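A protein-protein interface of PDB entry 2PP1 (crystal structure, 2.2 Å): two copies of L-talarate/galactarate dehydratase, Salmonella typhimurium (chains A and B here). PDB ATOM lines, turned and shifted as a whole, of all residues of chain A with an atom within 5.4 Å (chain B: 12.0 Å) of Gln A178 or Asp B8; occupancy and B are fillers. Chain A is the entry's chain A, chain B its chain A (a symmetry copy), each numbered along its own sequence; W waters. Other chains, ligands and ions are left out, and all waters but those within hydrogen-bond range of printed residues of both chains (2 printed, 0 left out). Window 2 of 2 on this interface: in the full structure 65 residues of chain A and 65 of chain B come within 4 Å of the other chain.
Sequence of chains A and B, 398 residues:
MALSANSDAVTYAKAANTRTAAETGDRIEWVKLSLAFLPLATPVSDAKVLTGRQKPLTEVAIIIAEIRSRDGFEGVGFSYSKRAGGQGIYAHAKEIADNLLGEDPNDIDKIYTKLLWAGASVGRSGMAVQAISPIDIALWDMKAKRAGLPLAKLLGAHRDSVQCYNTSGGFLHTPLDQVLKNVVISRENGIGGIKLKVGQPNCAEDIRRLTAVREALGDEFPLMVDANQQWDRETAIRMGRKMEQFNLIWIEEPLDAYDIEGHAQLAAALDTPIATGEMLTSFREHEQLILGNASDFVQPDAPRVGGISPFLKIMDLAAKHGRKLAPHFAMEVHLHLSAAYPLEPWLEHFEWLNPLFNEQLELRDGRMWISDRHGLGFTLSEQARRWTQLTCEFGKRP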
ATOM      1  N   THR A  42       2.298  18.577   0.307  1.00  0.00           N
ATOM      2  CA  THR A  42       2.627  17.295  -0.281  1.00  0.00           C
ATOM      3  C   THR A  42       4.135  17.055  -0.194  1.00  0.00           C
ATOM      4  O   THR A  42       4.907  17.703  -0.891  1.00  0.00           O
ATOM      5  CB  THR A  42       2.182  17.240  -1.762  1.00  0.00           C
ATOM      6  OG1 THR A  42       0.754  17.351  -1.839  1.00  0.00           O
ATOM      7  CG2 THR A  42       2.625  15.929  -2.409  1.00  0.00           C
ATOM      8  N   GLY A 169       6.092  19.476 -11.236  1.00  0.00           N
ATOM      9  CA  GLY A 169       5.148  18.433 -11.598  1.00  0.00           C
ATOM     10  C   GLY A 169       5.786  17.136 -12.080  1.00  0.00           C
ATOM     11  O   GLY A 169       5.090  16.253 -12.586  1.00  0.00           O
ATOM     12  N   THR A 174       5.459  11.241  -7.306  1.00  0.00           N
ATOM     13  CA  THR A 174       4.253  11.363  -8.120  1.00  0.00           C
ATOM     14  C   THR A 174       4.059  10.189  -9.084  1.00  0.00           C
ATOM     15  O   THR A 174       4.930   9.904  -9.909  1.00  0.00           O
ATOM     16  CB  THR A 174       4.305  12.652  -8.950  1.00  0.00           C
ATOM     17  OG1 THR A 174       4.567  13.766  -8.082  1.00  0.00           O
ATOM     18  CG2 THR A 174       2.994  12.859  -9.703  1.00  0.00           C
ATOM     19  N   PRO A 175       2.908   9.496  -8.999  1.00  0.00           N
ATOM     20  CA  PRO A 175       2.629   8.360  -9.883  1.00  0.00           C
ATOM     21  C   PRO A 175       2.618   8.824 -11.337  1.00  0.00           C
ATOM     22  O   PRO A 175       2.203   9.946 -11.625  1.00  0.00           O
ATOM     23  CB  PRO A 175       1.254   7.893  -9.420  1.00  0.00           C
ATOM     24  CG  PRO A 175       1.257   8.250  -7.957  1.00  0.00           C
ATOM     25  CD  PRO A 175       1.848   9.638  -7.986  1.00  0.00           C
ATOM     26  N   LEU A 176       3.075   7.967 -12.247  1.00  0.00           N
ATOM     27  CA  LEU A 176       3.119   8.313 -13.664  1.00  0.00           C
ATOM     28  C   LEU A 176       1.809   8.929 -14.141  1.00  0.00           C
ATOM     29  O   LEU A 176       1.806   9.902 -14.894  1.00  0.00           O
ATOM     30  CB  LEU A 176       3.439   7.074 -14.504  1.00  0.00           C
ATOM     31  CG  LEU A 176       3.493   7.297 -16.023  1.00  0.00           C
ATOM     32  CD1 LEU A 176       4.490   8.405 -16.356  1.00  0.00           C
ATOM     33  CD2 LEU A 176       3.891   6.000 -16.718  1.00  0.00           C
ATOM     34  N   ASP A 177       0.697   8.355 -13.696  1.00  0.00           N
ATOM     35  CA  ASP A 177      -0.620   8.853 -14.072  1.00  0.00           C
ATOM     36  C   ASP A 177      -0.772  10.344 -13.775  1.00  0.00           C
ATOM     37  O   ASP A 177      -1.199  11.119 -14.635  1.00  0.00           O
ATOM     38  CB  ASP A 177      -1.707   8.061 -13.336  1.00  0.00           C
ATOM     39  CG  ASP A 177      -3.078   8.716 -13.444  1.00  0.00           C
ATOM     40  OD1 ASP A 177      -3.338   9.713 -12.725  1.00  0.00           O
ATOM     41  OD2 ASP A 177      -3.896   8.240 -14.260  1.00  0.00           O
ATOM     42  N   GLN A 178      -0.427  10.733 -12.554  1.00  0.00           N
ATOM     43  CA  GLN A 178      -0.525  12.127 -12.129  1.00  0.00           C
ATOM     44  C   GLN A 178       0.491  13.004 -12.866  1.00  0.00           C
ATOM     45  O   GLN A 178       0.213  14.165 -13.163  1.00  0.00           O
ATOM     46  CB  GLN A 178      -0.320  12.222 -10.611  1.00  0.00           C
ATOM     47  CG  GLN A 178      -0.405  13.625 -10.047  1.00  0.00           C
ATOM     48  CD  GLN A 178      -1.750  14.277 -10.310  1.00  0.00           C
ATOM     49  OE1 GLN A 178      -1.840  15.267 -11.045  1.00  0.00           O
ATOM     50  NE2 GLN A 178      -2.803  13.723  -9.717  1.00  0.00           N
ATOM     51  N   VAL A 179       1.663  12.444 -13.170  1.00  0.00           N
ATOM     52  CA  VAL A 179       2.691  13.198 -13.887  1.00  0.00           C
ATOM     53  C   VAL A 179       2.161  13.593 -15.268  1.00  0.00           C
ATOM     54  O   VAL A 179       2.366  14.713 -15.723  1.00  0.00           O
ATOM     55  CB  VAL A 179       3.996  12.374 -14.071  1.00  0.00           C
ATOM     56  CG1 VAL A 179       4.983  13.145 -14.950  1.00  0.00           C
ATOM     57  CG2 VAL A 179       4.625  12.073 -12.721  1.00  0.00           C
ATOM     58  N   LEU A 180       1.479  12.663 -15.930  1.00  0.00           N
ATOM     59  CA  LEU A 180       0.908  12.935 -17.249  1.00  0.00           C
ATOM     60  C   LEU A 180      -0.177  14.005 -17.160  1.00  0.00           C
ATOM     61  O   LEU A 180      -0.337  14.813 -18.085  1.00  0.00           O
ATOM     62  CB  LEU A 180       0.345  11.653 -17.855  1.00  0.00           C
ATOM     63  CG  LEU A 180       1.432  10.623 -18.177  1.00  0.00           C
ATOM     64  CD1 LEU A 180       0.799   9.328 -18.636  1.00  0.00           C
ATOM     65  CD2 LEU A 180       2.349  11.171 -19.255  1.00  0.00           C
ATOM     66  N   LYS A 181      -0.912  14.009 -16.050  1.00  0.00           N
ATOM     67  CA  LYS A 181      -1.941  15.018 -15.822  1.00  0.00           C
ATOM     68  C   LYS A 181      -1.255  16.376 -15.616  1.00  0.00           C
ATOM     69  O   LYS A 181      -1.733  17.408 -16.104  1.00  0.00           O
ATOM     70  CB  LYS A 181      -2.766  14.682 -14.577  1.00  0.00           C
ATOM     71  CG  LYS A 181      -3.791  13.569 -14.754  1.00  0.00           C
ATOM     72  CD  LYS A 181      -4.476  13.280 -13.423  1.00  0.00           C
ATOM     73  CE  LYS A 181      -5.674  12.344 -13.582  1.00  0.00           C
ATOM     74  NZ  LYS A 181      -5.301  11.050 -14.219  1.00  0.00           N
ATOM     75  N   ASN A 182      -0.133  16.371 -14.893  1.00  0.00           N
ATOM     76  CA  ASN A 182       0.600  17.604 -14.622  1.00  0.00           C
ATOM     77  C   ASN A 182       1.124  18.210 -15.915  1.00  0.00           C
ATOM     78  O   ASN A 182       1.060  19.424 -16.110  1.00  0.00           O
ATOM     79  CB  ASN A 182       1.767  17.347 -13.669  1.00  0.00           C
ATOM     80  CG  ASN A 182       1.306  16.921 -12.273  1.00  0.00           C
ATOM     81  OD1 ASN A 182       0.229  17.307 -11.818  1.00  0.00           O
ATOM     82  ND2 ASN A 182       2.137  16.142 -11.583  1.00  0.00           N
ATOM     83  N   VAL A 183       1.639  17.361 -16.799  1.00  0.00           N
ATOM     84  CA  VAL A 183       2.160  17.829 -18.076  1.00  0.00           C
ATOM     85  C   VAL A 183       1.100  18.639 -18.810  1.00  0.00           C
ATOM     86  O   VAL A 183       1.393  19.690 -19.378  1.00  0.00           O
ATOM     87  CB  VAL A 183       2.590  16.651 -18.979  1.00  0.00           C
ATOM     88  CG1 VAL A 183       2.931  17.165 -20.366  1.00  0.00           C
ATOM     89  CG2 VAL A 183       3.793  15.937 -18.375  1.00  0.00           C
ATOM     90  N   ILE A 185      -1.667  20.116 -17.429  1.00  0.00           N
ATOM     91  CA  ILE A 185      -1.954  21.331 -16.677  1.00  0.00           C
ATOM     92  C   ILE A 185      -0.899  22.398 -16.989  1.00  0.00           C
ATOM     93  O   ILE A 185      -1.222  23.556 -17.258  1.00  0.00           O
ATOM     94  CB  ILE A 185      -1.939  21.069 -15.152  1.00  0.00           C
ATOM     95  CG1 ILE A 185      -3.052  20.088 -14.781  1.00  0.00           C
ATOM     96  CG2 ILE A 185      -2.090  22.390 -14.391  1.00  0.00           C
ATOM     97  CD1 ILE A 185      -3.071  19.722 -13.314  1.00  0.00           C
ATOM     98  N   SER B   4      -1.260  27.452  -0.033  1.00  0.00           N
ATOM     99  CA  SER B   4      -0.343  26.267   0.014  1.00  0.00           C
ATOM    100  C   SER B   4       0.770  26.402  -1.007  1.00  0.00           C
ATOM    101  O   SER B   4       0.548  26.850  -2.142  1.00  0.00           O
ATOM    102  CB  SER B   4      -1.103  24.968  -0.272  1.00  0.00           C
ATOM    103  OG  SER B   4      -1.439  24.865  -1.648  1.00  0.00           O
ATOM    104  N   ALA B   5       1.969  25.999  -0.606  1.00  0.00           N
ATOM    105  CA  ALA B   5       3.110  26.089  -1.493  1.00  0.00           C
ATOM    106  C   ALA B   5       2.993  25.091  -2.637  1.00  0.00           C
ATOM    107  O   ALA B   5       3.392  25.391  -3.762  1.00  0.00           O
ATOM    108  CB  ALA B   5       4.395  25.856  -0.714  1.00  0.00           C
ATOM    109  N   ASN B   6       2.441  23.909  -2.364  1.00  0.00           N
ATOM    110  CA  ASN B   6       2.309  22.897  -3.410  1.00  0.00           C
ATOM    111  C   ASN B   6       1.133  21.947  -3.191  1.00  0.00           C
ATOM    112  O   ASN B   6       0.373  22.103  -2.236  1.00  0.00           O
ATOM    113  CB  ASN B   6       3.615  22.098  -3.532  1.00  0.00           C
ATOM    114  CG  ASN B   6       3.751  21.014  -2.468  1.00  0.00           C
ATOM    115  OD1 ASN B   6       3.198  21.124  -1.372  1.00  0.00           O
ATOM    116  ND2 ASN B   6       4.506  19.963  -2.788  1.00  0.00           N
ATOM    117  N   SER B   7       0.994  20.973  -4.091  1.00  0.00           N
ATOM    118  CA  SER B   7      -0.078  19.979  -4.027  1.00  0.00           C
ATOM    119  C   SER B   7       0.385  18.709  -4.725  1.00  0.00           C
ATOM    120  O   SER B   7       1.543  18.604  -5.109  1.00  0.00           O
ATOM    121  CB  SER B   7      -1.335  20.502  -4.726  1.00  0.00           C
ATOM    122  OG  SER B   7      -1.114  20.657  -6.121  1.00  0.00           O
ATOM    123  N   ASP B   8      -0.522  17.754  -4.898  1.00  0.00           N
ATOM    124  CA  ASP B   8      -0.184  16.499  -5.562  1.00  0.00           C
ATOM    125  C   ASP B   8      -0.001  16.691  -7.058  1.00  0.00           C
ATOM    126  O   ASP B   8       0.613  15.864  -7.716  1.00  0.00           O
ATOM    127  CB  ASP B   8      -1.272  15.446  -5.341  1.00  0.00           C
ATOM    128  CG  ASP B   8      -1.417  15.053  -3.897  1.00  0.00           C
ATOM    129  OD1 ASP B   8      -0.480  15.303  -3.113  1.00  0.00           O
ATOM    130  OD2 ASP B   8      -2.470  14.478  -3.550  1.00  0.00           O
ATOM    131  N   ALA B   9      -0.554  17.771  -7.593  1.00  0.00           N
ATOM    132  CA  ALA B   9      -0.439  18.063  -9.015  1.00  0.00           C
ATOM    133  C   ALA B   9       0.499  19.253  -9.167  1.00  0.00           C
ATOM    134  O   ALA B   9       1.555  19.312  -8.531  1.00  0.00           O
ATOM    135  CB  ALA B   9      -1.830  18.389  -9.601  1.00  0.00           C
ATOM    136  N   VAL B  10       0.118  20.203 -10.009  1.00  0.00           N
ATOM    137  CA  VAL B  10       0.915  21.402 -10.203  1.00  0.00           C
ATOM    138  C   VAL B  10      -0.054  22.551 -10.450  1.00  0.00           C
ATOM    139  O   VAL B  10      -1.079  22.367 -11.095  1.00  0.00           O
ATOM    140  CB  VAL B  10       1.889  21.254 -11.408  1.00  0.00           C
ATOM    141  CG1 VAL B  10       1.122  20.922 -12.673  1.00  0.00           C
ATOM    142  CG2 VAL B  10       2.685  22.540 -11.591  1.00  0.00           C
ATOM    143  N   THR B  11       0.251  23.726  -9.916  1.00  0.00           N
ATOM    144  CA  THR B  11      -0.618  24.882 -10.116  1.00  0.00           C
ATOM    145  C   THR B  11       0.183  26.088 -10.600  1.00  0.00           C
ATOM    146  O   THR B  11       1.398  26.159 -10.414  1.00  0.00           O
ATOM    147  CB  THR B  11      -1.374  25.244  -8.827  1.00  0.00           C
ATOM    148  OG1 THR B  11      -0.458  25.268  -7.735  1.00  0.00           O
ATOM    149  CG2 THR B  11      -2.465  24.221  -8.540  1.00  0.00           C
ATOM    150  N   TYR B  12      -0.499  27.035 -11.225  1.00  0.00           N
ATOM    151  CA  TYR B  12       0.162  28.212 -11.756  1.00  0.00           C
ATOM    152  C   TYR B  12      -0.484  29.509 -11.295  1.00  0.00           C
ATOM    153  O   TYR B  12      -1.701  29.673 -11.377  1.00  0.00           O
ATOM    154  CB  TYR B  12       0.169  28.140 -13.288  1.00  0.00           C
ATOM    155  CG  TYR B  12       1.123  27.098 -13.825  1.00  0.00           C
ATOM    156  CD1 TYR B  12       2.435  27.438 -14.156  1.00  0.00           C
ATOM    157  CD2 TYR B  12       0.743  25.760 -13.932  1.00  0.00           C
ATOM    158  CE1 TYR B  12       3.348  26.476 -14.578  1.00  0.00           C
ATOM    159  CE2 TYR B  12       1.659  24.779 -14.350  1.00  0.00           C
ATOM    160  CZ  TYR B  12       2.963  25.151 -14.667  1.00  0.00           C
ATOM    161  OH  TYR B  12       3.900  24.201 -15.037  1.00  0.00           O
HETATM  162  O   HOH W   1       3.017  16.940  -8.583  1.00  0.00           O
HETATM  163  O   HOH W   2       2.150  14.001  -6.499  1.00  0.00           O
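Of chain B, only Asn B6 (3.0 Å), Ser B7 (3.2 Å) and Asp B8 (2.7 Å) come within 4 Å of Thr A42. No residue of chain B comes within 4 Å of Gly A169. No residue of chain B comes within 4 Å of Thr A174. No residue of chain B comes within 4 Å of Pro A175. Leu A176 touches none of the printed residues of chain B. No residue of chain B comes within 4 Å of Asp A177. Gln A178 touches two residues of chain B. No residue of chain B comes within 4 Å of Val A179. No residue of chain B comes within 4 Å of Leu A180. No residue of chain B comes within 4 Å of Lys A181. Of chain B, only Ala B9 (3.0 Å) and Val B10 (3.4 Å) come within 4 Å of Asn A182. Val A183 touches none of the printed residues of chain B. Printed residues of chain B within 4 Å of Ile A185: Val B10. Of the printed residues of chain A, Asn B6 touches Thr A42 (3.0 Å). Of the printed residues of chain A, Ser B7 touches Thr A42 (3.2 Å). Asp B8 touches just these residues of chain A: Thr A42 and Gln A178. Printed residues of chain A within 4 Å of Ala B9: Gln A178 (3.4 Å) and Asn A182 (3.0 Å). Thr B11 touches none of the printed residues of chain A. The nearest residue of chain B that does not touch Gln A178 is Val B10 (5.4 Å). The nearest printed residue of chain A that does not touch Ala B9 is Ile A185 (4.1 Å).
Of the 9 printed residues of chain B, 5 touch a printed residue of chain A. Printed residues of chain B that touch a printed residue of chain A: Asn B6, Ser B7, Asp B8, Ala B9 and Val B10. Of the 13 printed residues of chain A, 4 touch a printed residue of chain B. Printed residues of chain A that touch a printed residue of chain B: Thr A42, Gln A178, Asn A182 and Ile A185. Hydrophobic or aromatic side chains of chain A within 4 Å of the printed part of chain B: Ile A185. Among the printed residues, no Asp or Glu carboxylate lies within 4 Å of a Lys or Arg side-chain nitrogen of the other chain.
O of Thr A42 is in hydrogen-bond range of ND2 of Asn B6 (3.0 Å). The side-chain hydroxyl (OG1) of Thr A42 lies within hydrogen-bond range of the side-chain carboxylate (OD1) of Asp B8. The side-chain amide oxygen (OD1) of Asn A182 is in hydrogen-bond range of the backbone NH (N) of Val B10, 3.4 Å away.
Water W2 bridges the backbone carbonyl oxygen of Asp B8 (2.7 Å) and the side-chain hydroxyl of Thr A174 (2.9 Å). Water W1 lies within hydrogen-bond range of O of Asp B8 (2.8 Å), O of Ala B9 (2.8 Å) and ND2 of Asn A182 (3.2 Å).
Ser B7 touches Thr A42. O of Asp B8 touches CG of Gln A178 (3.4 Å). Gln A178 touches Ala B9. Asn A182 touches Ala B9 (OD1 to CA, 3.0 Å). Val B10 touches Ile A185.
The side-chain amide nitrogen (ND2) of Asn A182 lies within hydrogen-bond range of the backbone carbonyl oxygen (O) of Gly A169 (3.1 Å). OD1 of Asn A182 sits close to OE1 of Gln A178, at 3.0 Å. OG of Ser B4 is in hydrogen-bond range of O of Asn B6 (3.4 Å). OG of Ser B7 lies close to N of Ala B9, 3.3 Å away.
No position is printed for both chains. Of the 8 pairs that touch across the chains among the printed residues, none has its exchanged pair printed and touching as well.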
